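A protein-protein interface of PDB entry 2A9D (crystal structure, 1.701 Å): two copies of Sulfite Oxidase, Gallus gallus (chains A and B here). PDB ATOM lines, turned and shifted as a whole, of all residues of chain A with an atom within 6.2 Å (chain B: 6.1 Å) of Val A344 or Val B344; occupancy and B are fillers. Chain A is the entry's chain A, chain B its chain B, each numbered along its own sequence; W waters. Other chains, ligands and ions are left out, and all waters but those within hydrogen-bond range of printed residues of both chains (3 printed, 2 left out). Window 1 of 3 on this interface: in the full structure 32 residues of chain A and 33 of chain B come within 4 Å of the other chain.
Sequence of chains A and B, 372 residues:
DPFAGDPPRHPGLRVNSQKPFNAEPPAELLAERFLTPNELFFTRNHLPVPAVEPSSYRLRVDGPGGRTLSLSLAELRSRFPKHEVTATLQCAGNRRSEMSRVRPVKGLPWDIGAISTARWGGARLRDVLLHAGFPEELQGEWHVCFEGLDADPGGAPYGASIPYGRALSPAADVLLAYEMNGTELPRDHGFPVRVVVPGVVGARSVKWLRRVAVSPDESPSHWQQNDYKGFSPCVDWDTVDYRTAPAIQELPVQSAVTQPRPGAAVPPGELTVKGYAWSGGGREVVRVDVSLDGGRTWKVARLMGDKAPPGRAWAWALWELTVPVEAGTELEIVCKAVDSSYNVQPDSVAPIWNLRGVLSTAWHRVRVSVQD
Of the 13 printed residues of chain A, 6 touch a printed residue of chain B. Printed residues of chain A that touch a printed residue of chain B: Pro A252, Val A253, Tyr A342, Asn A343, Val A344 and Pro A346. Printed residues of chain B that touch a printed residue of chain A: Pro B252, Val B253, Tyr B342, Asn B343, Val B344, Gln B345 and Pro B346. Among the printed residues, 12 pairs touch across the chains.
The side-chain amide nitrogen (ND2) of Asn B343 sits close to the side-chain amide nitrogen (ND2) of Asn A343 (3.1 Å). The backbone NH (N) of Val B253 is in hydrogen-bond range of the side-chain amide oxygen (OD1) of Asn A343, 3.5 Å away.
Pro A252 touches Tyr B342, and with the chains exchanged Tyr A342 touches Pro B252. Val A253 touches Asn B343, and with the chains exchanged Asn A343 touches Val B253. Asn B343 touches its own counterpart, Asn A343. Val B344 touches its own counterpart, Val A344. Of the 12 pairs that touch across the chains among the printed residues, 11 have their exchanged pair printed and touching as well.
The side-chain amide nitrogen of Gln B345 lies within hydrogen-bond range of the backbone carbonyl oxygen of Thr B361. N of Tyr B342 sits at hydrogen-bond distance from OD1 of Asp B339. The backbone NH (N) of Asn A343 sits at hydrogen-bond distance from the side-chain carboxylate (OD1) of Asp A339 (3.0 Å). OD1 of Asp A339 lies within hydrogen-bond range of N of Tyr A342. The side-chain carboxylate (OD1) of Asp B339 lies within hydrogen-bond range of the backbone NH (N) of Asn B343, at 3.1 Å. N of Ala B337 lies within hydrogen-bond range of OE1 of Gln B345.
Printed residues of chain B within 4 Å of Pro A252: Tyr B342 (3.3 Å) and Asn B343 (3.6 Å). Of the printed residues of chain B, Tyr A342 touches Pro B252 (3.3 Å). Of the printed residues of chain B, Val A344 touches Val B344 and Pro B346. Printed residues of chain B within 4 Å of Pro A346: Val B344, Gln B345 and Pro B346. Of the printed residues of chain A, Val B253 touches Asn A343 (3.5 Å). Val B344 touches just these residues of chain A: Val A344 and Pro A346. Printed residues of chain A within 4 Å of Gln B345: Pro A346. The nearest residue of chain B that does not touch Val A344 is Ile B352 (4.4 Å). The nearest residue of chain A that does not touch Val B344 is Ile A352 (4.3 Å). The nearest printed residue of chain B that does not touch Val A253 is Tyr B342 (6.3 Å).
Pro A252 touches Tyr B342 (CB to O, 3.3 Å). CB of Pro A252 touches OD1 of Asn B343, at 3.6 Å. Val A253 touches Asn B343. Pro B252 touches Tyr A342. Pro B252 touches Asn A343 (CB to OD1, 3.2 Å). Val B344 touches Val A344. Val A344 touches Pro B346 (CG2 to CG, 3.7 Å). Pro A346 touches Val B344 (CG to CG2, 3.6 Å). Pro A346 touches Gln B345. Pro B346 touches Pro A346.
Water W2 lies within hydrogen-bond range of OD1 of Asn A343, O of Val B344 and N of Val A344. Water W3 bridges O of Val B344 (2.8 Å) and O of Val A344 (2.9 Å). Water W1 lies within hydrogen-bond range of O of Val A344 (2.9 Å), N of Val B344 (3.0 Å) and OD1 of Asn B343 (3.0 Å).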
ATOM      1  N   PRO A 252      28.533  -1.529 -15.177  1.00  0.00           N
ATOM      2  CA  PRO A 252      27.243  -0.836 -15.082  1.00  0.00           C
ATOM      3  C   PRO A 252      27.415   0.623 -14.620  1.00  0.00           C
ATOM      4  O   PRO A 252      28.482   1.004 -14.175  1.00  0.00           O
ATOM      5  CB  PRO A 252      26.507  -1.638 -14.014  1.00  0.00           C
ATOM      6  CG  PRO A 252      27.556  -2.194 -13.132  1.00  0.00           C
ATOM      7  CD  PRO A 252      28.747  -2.445 -14.036  1.00  0.00           C
ATOM      8  N   VAL A 253      26.342   1.392 -14.667  1.00  0.00           N
ATOM      9  CA  VAL A 253      26.384   2.800 -14.306  1.00  0.00           C
ATOM     10  C   VAL A 253      26.744   2.996 -12.825  1.00  0.00           C
ATOM     11  O   VAL A 253      26.371   2.198 -11.942  1.00  0.00           O
ATOM     12  CB  VAL A 253      25.048   3.504 -14.691  1.00  0.00           C
ATOM     13  CG1 VAL A 253      23.833   2.830 -14.040  1.00  0.00           C
ATOM     14  CG2 VAL A 253      25.020   4.966 -14.398  1.00  0.00           C
ATOM     15  N   LYS A 336      22.717   9.385  -7.631  1.00  0.00           N
ATOM     16  CA  LYS A 336      22.485   8.252  -8.528  1.00  0.00           C
ATOM     17  C   LYS A 336      22.485   8.761  -9.965  1.00  0.00           C
ATOM     18  O   LYS A 336      21.969   9.865 -10.269  1.00  0.00           O
ATOM     19  CB  LYS A 336      21.185   7.507  -8.220  1.00  0.00           C
ATOM     20  CG  LYS A 336      19.933   8.348  -8.358  1.00  0.00           C
ATOM     21  CD  LYS A 336      18.710   7.519  -7.963  1.00  0.00           C
ATOM     22  CE  LYS A 336      17.412   8.311  -8.020  1.00  0.00           C
ATOM     23  NZ  LYS A 336      16.899   8.454  -9.420  1.00  0.00           N
ATOM     24  N   ALA A 337      22.995   7.933 -10.855  1.00  0.00           N
ATOM     25  CA  ALA A 337      23.172   8.312 -12.260  1.00  0.00           C
ATOM     26  C   ALA A 337      22.364   7.438 -13.208  1.00  0.00           C
ATOM     27  O   ALA A 337      22.003   6.308 -12.890  1.00  0.00           O
ATOM     28  CB  ALA A 337      24.670   8.359 -12.643  1.00  0.00           C
ATOM     29  N   VAL A 338      22.110   8.011 -14.374  1.00  0.00           N
ATOM     30  CA  VAL A 338      21.312   7.376 -15.424  1.00  0.00           C
ATOM     31  C   VAL A 338      22.099   7.423 -16.723  1.00  0.00           C
ATOM     32  O   VAL A 338      22.633   8.473 -17.060  1.00  0.00           O
ATOM     33  CB  VAL A 338      19.989   8.122 -15.595  1.00  0.00           C
ATOM     34  CG1 VAL A 338      19.149   7.388 -16.596  1.00  0.00           C
ATOM     35  CG2 VAL A 338      19.262   8.162 -14.258  1.00  0.00           C
ATOM     36  N   ASP A 339      22.241   6.309 -17.434  1.00  0.00           N
ATOM     37  CA  ASP A 339      23.058   6.336 -18.658  1.00  0.00           C
ATOM     38  C   ASP A 339      22.193   6.346 -19.917  1.00  0.00           C
ATOM     39  O   ASP A 339      20.956   6.410 -19.849  1.00  0.00           O
ATOM     40  CB  ASP A 339      24.122   5.218 -18.686  1.00  0.00           C
ATOM     41  CG  ASP A 339      23.573   3.843 -18.986  1.00  0.00           C
ATOM     42  OD1 ASP A 339      22.399   3.694 -19.422  1.00  0.00           O
ATOM     43  OD2 ASP A 339      24.349   2.863 -18.859  1.00  0.00           O
ATOM     44  N   TYR A 342      19.272   4.235 -20.353  1.00  0.00           N
ATOM     45  CA  TYR A 342      18.418   4.406 -19.191  1.00  0.00           C
ATOM     46  C   TYR A 342      18.644   3.331 -18.121  1.00  0.00           C
ATOM     47  O   TYR A 342      17.762   3.019 -17.330  1.00  0.00           O
ATOM     48  CB  TYR A 342      16.953   4.584 -19.592  1.00  0.00           C
ATOM     49  CG  TYR A 342      16.668   5.981 -20.122  1.00  0.00           C
ATOM     50  CD1 TYR A 342      16.447   7.046 -19.241  1.00  0.00           C
ATOM     51  CD2 TYR A 342      16.616   6.231 -21.482  1.00  0.00           C
ATOM     52  CE1 TYR A 342      16.212   8.336 -19.724  1.00  0.00           C
ATOM     53  CE2 TYR A 342      16.366   7.535 -21.978  1.00  0.00           C
ATOM     54  CZ  TYR A 342      16.205   8.575 -21.088  1.00  0.00           C
ATOM     55  OH  TYR A 342      15.859   9.855 -21.563  1.00  0.00           O
ATOM     56  N   ASN A 343      19.883   2.839 -18.032  1.00  0.00           N
ATOM     57  CA  ASN A 343      20.218   1.976 -16.912  1.00  0.00           C
ATOM     58  C   ASN A 343      20.413   2.892 -15.694  1.00  0.00           C
ATOM     59  O   ASN A 343      20.774   4.049 -15.821  1.00  0.00           O
ATOM     60  CB  ASN A 343      21.385   1.024 -17.224  1.00  0.00           C
ATOM     61  CG  ASN A 343      20.900  -0.281 -17.865  1.00  0.00           C
ATOM     62  OD1 ASN A 343      20.176  -1.028 -17.240  1.00  0.00           O
ATOM     63  ND2 ASN A 343      21.106  -0.433 -19.173  1.00  0.00           N
ATOM     64  N   VAL A 344      20.020   2.378 -14.528  1.00  0.00           N
ATOM     65  CA  VAL A 344      20.021   3.110 -13.255  1.00  0.00           C
ATOM     66  C   VAL A 344      20.761   2.341 -12.163  1.00  0.00           C
ATOM     67  O   VAL A 344      21.105   1.165 -12.348  1.00  0.00           O
ATOM     68  CB  VAL A 344      18.558   3.344 -12.767  1.00  0.00           C
ATOM     69  CG1 VAL A 344      17.786   4.200 -13.771  1.00  0.00           C
ATOM     70  CG2 VAL A 344      17.817   2.030 -12.581  1.00  0.00           C
ATOM     71  N   GLN A 345      21.094   3.031 -11.075  1.00  0.00           N
ATOM     72  CA  GLN A 345      21.738   2.388  -9.933  1.00  0.00           C
ATOM     73  C   GLN A 345      20.695   1.931  -8.948  1.00  0.00           C
ATOM     74  O   GLN A 345      19.688   2.614  -8.748  1.00  0.00           O
ATOM     75  CB  GLN A 345      22.681   3.346  -9.235  1.00  0.00           C
ATOM     76  CG  GLN A 345      23.841   3.785 -10.105  1.00  0.00           C
ATOM     77  CD  GLN A 345      24.721   4.813  -9.394  1.00  0.00           C
ATOM     78  OE1 GLN A 345      24.703   6.020  -9.727  1.00  0.00           O
ATOM     79  NE2 GLN A 345      25.382   4.369  -8.330  1.00  0.00           N
ATOM     80  N   PRO A 346      20.959   0.798  -8.284  1.00  0.00           N
ATOM     81  CA  PRO A 346      20.018   0.304  -7.312  1.00  0.00           C
ATOM     82  C   PRO A 346      20.118   0.984  -5.947  1.00  0.00           C
ATOM     83  O   PRO A 346      21.190   1.488  -5.565  1.00  0.00           O
ATOM     84  CB  PRO A 346      20.385  -1.187  -7.226  1.00  0.00           C
ATOM     85  CG  PRO A 346      21.811  -1.219  -7.424  1.00  0.00           C
ATOM     86  CD  PRO A 346      22.123  -0.101  -8.404  1.00  0.00           C
ATOM     87  N   ILE A 352      22.877  -6.655  -4.032  1.00  0.00           N
ATOM     88  CA  ILE A 352      23.914  -6.769  -5.049  1.00  0.00           C
ATOM     89  C   ILE A 352      25.207  -7.321  -4.435  1.00  0.00           C
ATOM     90  O   ILE A 352      26.292  -7.297  -5.058  1.00  0.00           O
ATOM     91  CB  ILE A 352      24.200  -5.424  -5.785  1.00  0.00           C
ATOM     92  CG1 ILE A 352      24.651  -4.318  -4.805  1.00  0.00           C
ATOM     93  CG2 ILE A 352      22.974  -4.995  -6.636  1.00  0.00           C
ATOM     94  CD1 ILE A 352      25.404  -3.211  -5.525  1.00  0.00           C
ATOM     95  N   THR A 361      27.698  -0.720  -6.954  1.00  0.00           N
ATOM     96  CA  THR A 361      27.082   0.442  -7.604  1.00  0.00           C
ATOM     97  C   THR A 361      25.777   0.908  -6.953  1.00  0.00           C
ATOM     98  O   THR A 361      25.065   1.733  -7.542  1.00  0.00           O
ATOM     99  CB  THR A 361      26.819   0.170  -9.111  1.00  0.00           C
ATOM    100  OG1 THR A 361      25.792  -0.825  -9.226  1.00  0.00           O
ATOM    101  CG2 THR A 361      28.075  -0.248  -9.822  1.00  0.00           C
ATOM    102  N   PRO B 252      16.733  -0.484 -20.387  1.00  0.00           N
ATOM    103  CA  PRO B 252      17.435  -1.123 -19.313  1.00  0.00           C
ATOM    104  C   PRO B 252      16.909  -2.539 -18.988  1.00  0.00           C
ATOM    105  O   PRO B 252      15.810  -2.940 -19.399  1.00  0.00           O
ATOM    106  CB  PRO B 252      17.183  -0.177 -18.145  1.00  0.00           C
ATOM    107  CG  PRO B 252      15.869   0.426 -18.430  1.00  0.00           C
ATOM    108  CD  PRO B 252      15.850   0.600 -19.911  1.00  0.00           C
ATOM    109  N   VAL B 253      17.687  -3.250 -18.186  1.00  0.00           N
ATOM    110  CA  VAL B 253      17.379  -4.618 -17.778  1.00  0.00           C
ATOM    111  C   VAL B 253      16.017  -4.646 -17.024  1.00  0.00           C
ATOM    112  O   VAL B 253      15.671  -3.745 -16.222  1.00  0.00           O
ATOM    113  CB  VAL B 253      18.572  -5.242 -16.974  1.00  0.00           C
ATOM    114  CG1 VAL B 253      18.873  -4.419 -15.718  1.00  0.00           C
ATOM    115  CG2 VAL B 253      18.307  -6.707 -16.590  1.00  0.00           C
ATOM    116  N   ALA B 337      16.853  -9.206 -12.488  1.00  0.00           N
ATOM    117  CA  ALA B 337      17.747  -9.739 -13.504  1.00  0.00           C
ATOM    118  C   ALA B 337      19.034  -8.947 -13.640  1.00  0.00           C
ATOM    119  O   ALA B 337      19.075  -7.767 -13.290  1.00  0.00           O
ATOM    120  CB  ALA B 337      17.014  -9.794 -14.846  1.00  0.00           C
ATOM    121  N   VAL B 338      20.057  -9.618 -14.171  1.00  0.00           N
ATOM    122  CA  VAL B 338      21.399  -9.007 -14.385  1.00  0.00           C
ATOM    123  C   VAL B 338      21.800  -9.257 -15.833  1.00  0.00           C
ATOM    124  O   VAL B 338      21.619 -10.357 -16.324  1.00  0.00           O
ATOM    125  CB  VAL B 338      22.454  -9.652 -13.438  1.00  0.00           C
ATOM    126  CG1 VAL B 338      23.792  -9.008 -13.612  1.00  0.00           C
ATOM    127  CG2 VAL B 338      21.980  -9.601 -11.971  1.00  0.00           C
ATOM    128  N   ASP B 339      22.306  -8.244 -16.540  1.00  0.00           N
ATOM    129  CA  ASP B 339      22.617  -8.421 -17.958  1.00  0.00           C
ATOM    130  C   ASP B 339      24.130  -8.564 -18.162  1.00  0.00           C
ATOM    131  O   ASP B 339      24.905  -8.550 -17.203  1.00  0.00           O
ATOM    132  CB  ASP B 339      21.966  -7.349 -18.848  1.00  0.00           C
ATOM    133  CG  ASP B 339      22.631  -5.972 -18.781  1.00  0.00           C
ATOM    134  OD1 ASP B 339      23.762  -5.836 -18.268  1.00  0.00           O
ATOM    135  OD2 ASP B 339      22.001  -5.008 -19.314  1.00  0.00           O
ATOM    136  N   TYR B 342      26.462  -6.314 -16.552  1.00  0.00           N
ATOM    137  CA  TYR B 342      26.194  -6.352 -15.122  1.00  0.00           C
ATOM    138  C   TYR B 342      25.326  -5.174 -14.630  1.00  0.00           C
ATOM    139  O   TYR B 342      25.422  -4.755 -13.483  1.00  0.00           O
ATOM    140  CB  TYR B 342      27.463  -6.514 -14.305  1.00  0.00           C
ATOM    141  CG  TYR B 342      28.006  -7.928 -14.316  1.00  0.00           C
ATOM    142  CD1 TYR B 342      27.448  -8.899 -13.501  1.00  0.00           C
ATOM    143  CD2 TYR B 342      29.023  -8.298 -15.196  1.00  0.00           C
ATOM    144  CE1 TYR B 342      27.933 -10.199 -13.509  1.00  0.00           C
ATOM    145  CE2 TYR B 342      29.553  -9.590 -15.185  1.00  0.00           C
ATOM    146  CZ  TYR B 342      29.006 -10.530 -14.344  1.00  0.00           C
ATOM    147  OH  TYR B 342      29.538 -11.839 -14.281  1.00  0.00           O
ATOM    148  N   ASN B 343      24.479  -4.685 -15.514  1.00  0.00           N
ATOM    149  CA  ASN B 343      23.438  -3.765 -15.124  1.00  0.00           C
ATOM    150  C   ASN B 343      22.453  -4.560 -14.315  1.00  0.00           C
ATOM    151  O   ASN B 343      22.252  -5.754 -14.581  1.00  0.00           O
ATOM    152  CB  ASN B 343      22.691  -3.202 -16.292  1.00  0.00           C
ATOM    153  CG  ASN B 343      23.387  -2.098 -16.916  1.00  0.00           C
ATOM    154  OD1 ASN B 343      23.744  -1.107 -16.249  1.00  0.00           O
ATOM    155  ND2 ASN B 343      23.542  -2.203 -18.261  1.00  0.00           N
ATOM    156  N   VAL B 344      21.812  -3.884 -13.367  1.00  0.00           N
ATOM    157  CA  VAL B 344      20.873  -4.480 -12.428  1.00  0.00           C
ATOM    158  C   VAL B 344      19.608  -3.638 -12.322  1.00  0.00           C
ATOM    159  O   VAL B 344      19.585  -2.478 -12.745  1.00  0.00           O
ATOM    160  CB  VAL B 344      21.515  -4.617 -10.999  1.00  0.00           C
ATOM    161  CG1 VAL B 344      22.776  -5.512 -11.010  1.00  0.00           C
ATOM    162  CG2 VAL B 344      21.919  -3.280 -10.430  1.00  0.00           C
ATOM    163  N   GLN B 345      18.567  -4.241 -11.760  1.00  0.00           N
ATOM    164  CA  GLN B 345      17.285  -3.567 -11.492  1.00  0.00           C
ATOM    165  C   GLN B 345      17.284  -2.939 -10.095  1.00  0.00           C
ATOM    166  O   GLN B 345      17.801  -3.537  -9.144  1.00  0.00           O
ATOM    167  CB  GLN B 345      16.132  -4.556 -11.587  1.00  0.00           C
ATOM    168  CG  GLN B 345      15.902  -5.058 -12.983  1.00  0.00           C
ATOM    169  CD  GLN B 345      14.740  -6.023 -13.040  1.00  0.00           C
ATOM    170  OE1 GLN B 345      14.960  -7.226 -13.172  1.00  0.00           O
ATOM    171  NE2 GLN B 345      13.530  -5.538 -12.763  1.00  0.00           N
ATOM    172  N   PRO B 346      16.668  -1.744  -9.948  1.00  0.00           N
ATOM    173  CA  PRO B 346      16.654  -1.088  -8.642  1.00  0.00           C
ATOM    174  C   PRO B 346      15.565  -1.689  -7.745  1.00  0.00           C
ATOM    175  O   PRO B 346      14.489  -2.104  -8.237  1.00  0.00           O
ATOM    176  CB  PRO B 346      16.314   0.372  -8.979  1.00  0.00           C
ATOM    177  CG  PRO B 346      15.561   0.292 -10.230  1.00  0.00           C
ATOM    178  CD  PRO B 346      16.082  -0.907 -10.988  1.00  0.00           C
ATOM    179  N   ILE B 352      12.706   6.014  -9.292  1.00  0.00           N
ATOM    180  CA  ILE B 352      12.668   5.974 -10.753  1.00  0.00           C
ATOM    181  C   ILE B 352      11.329   6.496 -11.280  1.00  0.00           C
ATOM    182  O   ILE B 352      11.039   6.393 -12.467  1.00  0.00           O
ATOM    183  CB  ILE B 352      12.937   4.576 -11.329  1.00  0.00           C
ATOM    184  CG1 ILE B 352      11.960   3.503 -10.806  1.00  0.00           C
ATOM    185  CG2 ILE B 352      14.333   4.143 -11.011  1.00  0.00           C
ATOM    186  CD1 ILE B 352      11.877   2.298 -11.675  1.00  0.00           C
ATOM    187  N   THR B 361      11.212  -0.437 -14.155  1.00  0.00           N
ATOM    188  CA  THR B 361      12.050  -1.638 -14.026  1.00  0.00           C
ATOM    189  C   THR B 361      12.499  -1.963 -12.598  1.00  0.00           C
ATOM    190  O   THR B 361      13.412  -2.779 -12.410  1.00  0.00           O
ATOM    191  CB  THR B 361      13.330  -1.547 -14.901  1.00  0.00           C
ATOM    192  OG1 THR B 361      14.177  -0.525 -14.371  1.00  0.00           O
ATOM    193  CG2 THR B 361      12.998  -1.282 -16.312  1.00  0.00           C
HETATM  194  O   HOH W   1      22.628  -1.027 -13.429  1.00  0.00           O
HETATM  195  O   HOH W   2      19.312  -0.629 -14.820  1.00  0.00           O
HETATM  196  O   HOH W   3      19.523  -0.569 -10.641  1.00  0.00           O
